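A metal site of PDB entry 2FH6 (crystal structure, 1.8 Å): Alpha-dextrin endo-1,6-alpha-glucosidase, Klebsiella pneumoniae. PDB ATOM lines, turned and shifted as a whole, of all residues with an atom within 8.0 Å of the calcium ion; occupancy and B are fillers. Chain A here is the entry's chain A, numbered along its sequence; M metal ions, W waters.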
ATOM      1  N   THR A 484     -30.922  -8.688   7.264  1.00  0.00           N
ATOM      2  CA  THR A 484     -30.087  -9.676   6.592  1.00  0.00           C
ATOM      3  C   THR A 484     -29.647  -9.511   5.143  1.00  0.00           C
ATOM      4  O   THR A 484     -29.195 -10.477   4.522  1.00  0.00           O
ATOM      5  CB  THR A 484     -30.700 -11.055   6.787  1.00  0.00           C
ATOM      6  OG1 THR A 484     -32.096 -11.001   6.482  1.00  0.00           O
ATOM      7  CG2 THR A 484     -30.526 -11.512   8.233  1.00  0.00           C
ATOM      8  N   VAL A 485     -29.759  -8.302   4.608  1.00  0.00           N
ATOM      9  CA  VAL A 485     -29.292  -8.016   3.262  1.00  0.00           C
ATOM     10  C   VAL A 485     -28.570  -6.671   3.388  1.00  0.00           C
ATOM     11  O   VAL A 485     -29.126  -5.715   3.921  1.00  0.00           O
ATOM     12  CB  VAL A 485     -30.447  -7.880   2.242  1.00  0.00           C
ATOM     13  CG1 VAL A 485     -29.906  -7.355   0.914  1.00  0.00           C
ATOM     14  CG2 VAL A 485     -31.090  -9.260   2.010  1.00  0.00           C
ATOM     15  N   ASN A 486     -27.323  -6.612   2.924  1.00  0.00           N
ATOM     16  CA  ASN A 486     -26.565  -5.365   3.011  1.00  0.00           C
ATOM     17  C   ASN A 486     -27.122  -4.411   1.951  1.00  0.00           C
ATOM     18  O   ASN A 486     -27.176  -4.761   0.764  1.00  0.00           O
ATOM     19  CB  ASN A 486     -25.074  -5.623   2.772  1.00  0.00           C
ATOM     20  CG  ASN A 486     -24.223  -4.444   3.203  1.00  0.00           C
ATOM     21  OD1 ASN A 486     -24.558  -3.287   2.942  1.00  0.00           O
ATOM     22  ND2 ASN A 486     -23.099  -4.729   3.854  1.00  0.00           N
ATOM     23  N   ASP A 494     -24.468 -10.656  -6.736  1.00  0.00           N
ATOM     24  CA  ASP A 494     -25.547 -11.569  -7.068  1.00  0.00           C
ATOM     25  C   ASP A 494     -25.121 -12.524  -8.172  1.00  0.00           C
ATOM     26  O   ASP A 494     -24.124 -12.275  -8.863  1.00  0.00           O
ATOM     27  CB  ASP A 494     -26.801 -10.777  -7.446  1.00  0.00           C
ATOM     28  CG  ASP A 494     -27.470 -10.157  -6.235  1.00  0.00           C
ATOM     29  OD1 ASP A 494     -27.893 -10.932  -5.352  1.00  0.00           O
ATOM     30  OD2 ASP A 494     -27.559  -8.916  -6.146  1.00  0.00           O
ATOM     31  N   ASN A 546     -23.410 -22.194  -3.605  1.00  0.00           N
ATOM     32  CA  ASN A 546     -24.507 -21.306  -3.275  1.00  0.00           C
ATOM     33  C   ASN A 546     -24.521 -20.898  -1.809  1.00  0.00           C
ATOM     34  O   ASN A 546     -24.856 -19.758  -1.491  1.00  0.00           O
ATOM     35  CB  ASN A 546     -25.844 -21.946  -3.639  1.00  0.00           C
ATOM     36  CG  ASN A 546     -26.947 -20.916  -3.794  1.00  0.00           C
ATOM     37  OD1 ASN A 546     -26.816 -19.982  -4.579  1.00  0.00           O
ATOM     38  ND2 ASN A 546     -28.033 -21.080  -3.050  1.00  0.00           N
ATOM     39  N   THR A 547     -24.162 -21.815  -0.919  1.00  0.00           N
ATOM     40  CA  THR A 547     -24.135 -21.522   0.507  1.00  0.00           C
ATOM     41  C   THR A 547     -23.198 -20.342   0.778  1.00  0.00           C
ATOM     42  O   THR A 547     -23.450 -19.537   1.665  1.00  0.00           O
ATOM     43  CB  THR A 547     -23.686 -22.757   1.323  1.00  0.00           C
ATOM     44  OG1 THR A 547     -24.663 -23.804   1.166  1.00  0.00           O
ATOM     45  CG2 THR A 547     -23.566 -22.422   2.799  1.00  0.00           C
ATOM     46  N   LEU A 548     -22.131 -20.243  -0.011  1.00  0.00           N
ATOM     47  CA  LEU A 548     -21.166 -19.145   0.145  1.00  0.00           C
ATOM     48  C   LEU A 548     -21.742 -17.882  -0.498  1.00  0.00           C
ATOM     49  O   LEU A 548     -21.578 -16.774   0.028  1.00  0.00           O
ATOM     50  CB  LEU A 548     -19.831 -19.501  -0.516  1.00  0.00           C
ATOM     51  CG  LEU A 548     -19.154 -20.765   0.023  1.00  0.00           C
ATOM     52  CD1 LEU A 548     -17.826 -20.968  -0.690  1.00  0.00           C
ATOM     53  CD2 LEU A 548     -18.944 -20.645   1.526  1.00  0.00           C
ATOM     54  N   VAL A 549     -22.399 -18.056  -1.634  1.00  0.00           N
ATOM     55  CA  VAL A 549     -23.005 -16.931  -2.353  1.00  0.00           C
ATOM     56  C   VAL A 549     -24.064 -16.253  -1.481  1.00  0.00           C
ATOM     57  O   VAL A 549     -24.195 -15.023  -1.469  1.00  0.00           O
ATOM     58  CB  VAL A 549     -23.710 -17.417  -3.652  1.00  0.00           C
ATOM     59  CG1 VAL A 549     -24.451 -16.255  -4.303  1.00  0.00           C
ATOM     60  CG2 VAL A 549     -22.667 -18.005  -4.612  1.00  0.00           C
ATOM     61  N   ALA A 550     -24.814 -17.076  -0.741  1.00  0.00           N
ATOM     62  CA  ALA A 550     -25.883 -16.585   0.118  1.00  0.00           C
ATOM     63  C   ALA A 550     -25.466 -15.550   1.157  1.00  0.00           C
ATOM     64  O   ALA A 550     -26.273 -14.695   1.557  1.00  0.00           O
ATOM     65  CB  ALA A 550     -26.545 -17.774   0.817  1.00  0.00           C
ATOM     66  N   GLN A 551     -24.211 -15.603   1.585  1.00  0.00           N
ATOM     67  CA  GLN A 551     -23.677 -14.699   2.604  1.00  0.00           C
ATOM     68  C   GLN A 551     -23.608 -13.240   2.162  1.00  0.00           C
ATOM     69  O   GLN A 551     -23.723 -12.330   2.982  1.00  0.00           O
ATOM     70  CB  GLN A 551     -22.273 -15.149   3.020  1.00  0.00           C
ATOM     71  CG  GLN A 551     -22.189 -16.569   3.536  1.00  0.00           C
ATOM     72  CD  GLN A 551     -20.755 -17.069   3.620  1.00  0.00           C
ATOM     73  OE1 GLN A 551     -20.497 -18.140   4.180  1.00  0.00           O
ATOM     74  NE2 GLN A 551     -19.830 -16.306   3.057  1.00  0.00           N
ATOM     75  N   THR A 552     -23.426 -13.026   0.865  1.00  0.00           N
ATOM     76  CA  THR A 552     -23.273 -11.671   0.360  1.00  0.00           C
ATOM     77  C   THR A 552     -24.162 -11.297  -0.823  1.00  0.00           C
ATOM     78  O   THR A 552     -23.839 -10.361  -1.563  1.00  0.00           O
ATOM     79  CB  THR A 552     -21.795 -11.428  -0.023  1.00  0.00           C
ATOM     80  OG1 THR A 552     -21.314 -12.513  -0.819  1.00  0.00           O
ATOM     81  CG2 THR A 552     -20.931 -11.325   1.232  1.00  0.00           C
ATOM     82  N   ASP A 553     -25.270 -12.002  -1.012  1.00  0.00           N
ATOM     83  CA  ASP A 553     -26.166 -11.670  -2.118  1.00  0.00           C
ATOM     84  C   ASP A 553     -27.293 -10.746  -1.640  1.00  0.00           C
ATOM     85  O   ASP A 553     -27.293 -10.285  -0.498  1.00  0.00           O
ATOM     86  CB  ASP A 553     -26.752 -12.940  -2.769  1.00  0.00           C
ATOM     87  CG  ASP A 553     -27.564 -13.788  -1.805  1.00  0.00           C
ATOM     88  OD1 ASP A 553     -27.891 -13.315  -0.693  1.00  0.00           O
ATOM     89  OD2 ASP A 553     -27.908 -14.940  -2.170  1.00  0.00           O
ATOM     90  N   SER A 554     -28.248 -10.480  -2.524  1.00  0.00           N
ATOM     91  CA  SER A 554     -29.366  -9.591  -2.184  1.00  0.00           C
ATOM     92  C   SER A 554     -30.570 -10.378  -1.706  1.00  0.00           C
ATOM     93  O   SER A 554     -31.655  -9.816  -1.523  1.00  0.00           O
ATOM     94  CB  SER A 554     -29.775  -8.787  -3.425  1.00  0.00           C
ATOM     95  OG  SER A 554     -28.707  -8.005  -3.911  1.00  0.00           O
ATOM     96  N   TYR A 555     -30.394 -11.676  -1.467  1.00  0.00           N
ATOM     97  CA  TYR A 555     -31.509 -12.524  -1.078  1.00  0.00           C
ATOM     98  C   TYR A 555     -31.689 -12.981   0.366  1.00  0.00           C
ATOM     99  O   TYR A 555     -30.744 -13.413   1.025  1.00  0.00           O
ATOM    100  CB  TYR A 555     -31.503 -13.791  -1.963  1.00  0.00           C
ATOM    101  CG  TYR A 555     -32.823 -14.540  -1.940  1.00  0.00           C
ATOM    102  CD1 TYR A 555     -33.212 -15.280  -0.811  1.00  0.00           C
ATOM    103  CD2 TYR A 555     -33.707 -14.443  -2.998  1.00  0.00           C
ATOM    104  CE1 TYR A 555     -34.470 -15.877  -0.755  1.00  0.00           C
ATOM    105  CE2 TYR A 555     -34.962 -15.040  -2.956  1.00  0.00           C
ATOM    106  CZ  TYR A 555     -35.336 -15.751  -1.829  1.00  0.00           C
ATOM    107  OH  TYR A 555     -36.593 -16.312  -1.763  1.00  0.00           O
ATOM    108  N   ASN A 556     -32.937 -12.891   0.823  1.00  0.00           N
ATOM    109  CA  ASN A 556     -33.364 -13.346   2.134  1.00  0.00           C
ATOM    110  C   ASN A 556     -34.858 -13.097   2.269  1.00  0.00           C
ATOM    111  O   ASN A 556     -35.368 -12.088   1.776  1.00  0.00           O
ATOM    112  CB  ASN A 556     -32.626 -12.628   3.265  1.00  0.00           C
ATOM    113  CG  ASN A 556     -32.675 -13.404   4.566  1.00  0.00           C
ATOM    114  OD1 ASN A 556     -33.746 -13.578   5.159  1.00  0.00           O
ATOM    115  ND2 ASN A 556     -31.522 -13.905   5.006  1.00  0.00           N
ATOM    116  N   TRP A 557     -35.570 -14.019   2.918  1.00  0.00           N
ATOM    117  CA  TRP A 557     -36.996 -13.817   3.120  1.00  0.00           C
ATOM    118  C   TRP A 557     -37.207 -12.526   3.906  1.00  0.00           C
ATOM    119  O   TRP A 557     -38.168 -11.789   3.671  1.00  0.00           O
ATOM    120  CB  TRP A 557     -37.616 -14.970   3.899  1.00  0.00           C
ATOM    121  CG  TRP A 557     -37.831 -16.213   3.109  1.00  0.00           C
ATOM    122  CD1 TRP A 557     -37.802 -16.348   1.758  1.00  0.00           C
ATOM    123  CD2 TRP A 557     -38.128 -17.509   3.637  1.00  0.00           C
ATOM    124  NE1 TRP A 557     -38.055 -17.655   1.396  1.00  0.00           N
ATOM    125  CE2 TRP A 557     -38.261 -18.389   2.538  1.00  0.00           C
ATOM    126  CE3 TRP A 557     -38.288 -18.021   4.937  1.00  0.00           C
ATOM    127  CZ2 TRP A 557     -38.549 -19.747   2.698  1.00  0.00           C
ATOM    128  CZ3 TRP A 557     -38.571 -19.371   5.100  1.00  0.00           C
ATOM    129  CH2 TRP A 557     -38.700 -20.221   3.981  1.00  0.00           C
ATOM    130  N   SER A 891     -35.917 -22.473   2.485  1.00  0.00           N
ATOM    131  CA  SER A 891     -35.156 -21.679   1.534  1.00  0.00           C
ATOM    132  C   SER A 891     -34.907 -20.201   1.817  1.00  0.00           C
ATOM    133  O   SER A 891     -34.501 -19.473   0.912  1.00  0.00           O
ATOM    134  CB  SER A 891     -35.808 -21.801   0.152  1.00  0.00           C
ATOM    135  OG  SER A 891     -37.037 -21.094   0.099  1.00  0.00           O
ATOM    136  N   TYR A 892     -35.116 -19.768   3.055  1.00  0.00           N
ATOM    137  CA  TYR A 892     -34.960 -18.360   3.434  1.00  0.00           C
ATOM    138  C   TYR A 892     -33.665 -17.675   3.004  1.00  0.00           C
ATOM    139  O   TYR A 892     -33.654 -16.460   2.797  1.00  0.00           O
ATOM    140  CB  TYR A 892     -35.097 -18.185   4.955  1.00  0.00           C
ATOM    141  CG  TYR A 892     -33.846 -18.533   5.740  1.00  0.00           C
ATOM    142  CD1 TYR A 892     -33.412 -19.857   5.879  1.00  0.00           C
ATOM    143  CD2 TYR A 892     -33.085 -17.529   6.349  1.00  0.00           C
ATOM    144  CE1 TYR A 892     -32.262 -20.171   6.601  1.00  0.00           C
ATOM    145  CE2 TYR A 892     -31.935 -17.831   7.079  1.00  0.00           C
ATOM    146  CZ  TYR A 892     -31.527 -19.156   7.204  1.00  0.00           C
ATOM    147  OH  TYR A 892     -30.397 -19.463   7.914  1.00  0.00           O
ATOM    148  N   ASP A 893     -32.588 -18.435   2.888  1.00  0.00           N
ATOM    149  CA  ASP A 893     -31.288 -17.861   2.512  1.00  0.00           C
ATOM    150  C   ASP A 893     -30.672 -18.655   1.365  1.00  0.00           C
ATOM    151  O   ASP A 893     -29.453 -18.611   1.180  1.00  0.00           O
ATOM    152  CB  ASP A 893     -30.362 -17.892   3.732  1.00  0.00           C
ATOM    153  CG  ASP A 893     -29.195 -16.938   3.613  1.00  0.00           C
ATOM    154  OD1 ASP A 893     -28.236 -17.085   4.395  1.00  0.00           O
ATOM    155  OD2 ASP A 893     -29.229 -16.040   2.737  1.00  0.00           O
ATOM    156  N   SER A 894     -31.509 -19.358   0.613  1.00  0.00           N
ATOM    157  CA  SER A 894     -31.036 -20.175  -0.501  1.00  0.00           C
ATOM    158  C   SER A 894     -30.895 -19.430  -1.823  1.00  0.00           C
ATOM    159  O   SER A 894     -30.689 -20.046  -2.873  1.00  0.00           O
ATOM    160  CB  SER A 894     -31.937 -21.400  -0.677  1.00  0.00           C
ATOM    161  OG  SER A 894     -31.756 -22.281   0.424  1.00  0.00           O
ATOM    162  N   GLY A 895     -31.012 -18.107  -1.758  1.00  0.00           N
ATOM    163  CA  GLY A 895     -30.836 -17.249  -2.924  1.00  0.00           C
ATOM    164  C   GLY A 895     -31.751 -17.364  -4.127  1.00  0.00           C
ATOM    165  O   GLY A 895     -32.766 -18.055  -4.120  1.00  0.00           O
ATOM    166  N   ASP A 896     -31.376 -16.645  -5.188  1.00  0.00           N
ATOM    167  CA  ASP A 896     -32.116 -16.639  -6.439  1.00  0.00           C
ATOM    168  C   ASP A 896     -32.141 -18.029  -7.075  1.00  0.00           C
ATOM    169  O   ASP A 896     -33.096 -18.392  -7.753  1.00  0.00           O
ATOM    170  CB  ASP A 896     -31.489 -15.677  -7.454  1.00  0.00           C
ATOM    171  CG  ASP A 896     -31.593 -14.222  -7.048  1.00  0.00           C
ATOM    172  OD1 ASP A 896     -32.511 -13.872  -6.266  1.00  0.00           O
ATOM    173  OD2 ASP A 896     -30.760 -13.422  -7.524  1.00  0.00           O
HETATM  174 CA    CA M   1     -28.620 -14.109   1.485  1.00  0.00          CA
HETATM  175  O   HOH W   1     -28.975 -13.247   3.794  1.00  0.00           O
HETATM  176  O   HOH W   2     -27.906 -11.837   1.633  1.00  0.00           O
HETATM  177  O   HOH W   3     -29.162 -15.957  -0.111  1.00  0.00           O
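Water W2 lies within hydrogen-bond range of O of Asp 553 and O of Thr 484.
Water W1 lies within hydrogen-bond range of the backbone carbonyl oxygen of Thr 484 (2.9 Å) and the side-chain amide nitrogen of Asn 556 (2.9 Å).
Water W3 lies within hydrogen-bond range of the side-chain carboxylate (OD2) of Asp 553 (2.6 Å), the backbone carbonyl oxygen (O) of Asp 893 (3.0 Å) and the backbone NH (N) of Gly 895 (3.3 Å).
Within 4 Å of the calcium ion: Ala 550, Asp 553, Tyr 555 and Asp 893.
O of Tyr 555 is bound to the calcium ion (2.3 Å).
The side-chain carboxylate (OD2) of Asp 893 is bound to the calcium ion (2.4 Å).
The calcium ion is bound by water W2.
O of Ala 550 is bound to the calcium ion, at 2.4 Å.
OD1 of Asp 553 is bound to the calcium ion, 2.4 Å away.
The calcium ion is bound by water W1.
The calcium ion is bound by water W3 (2.5 Å).
The calcium ion has seven donor atoms within binding distance.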
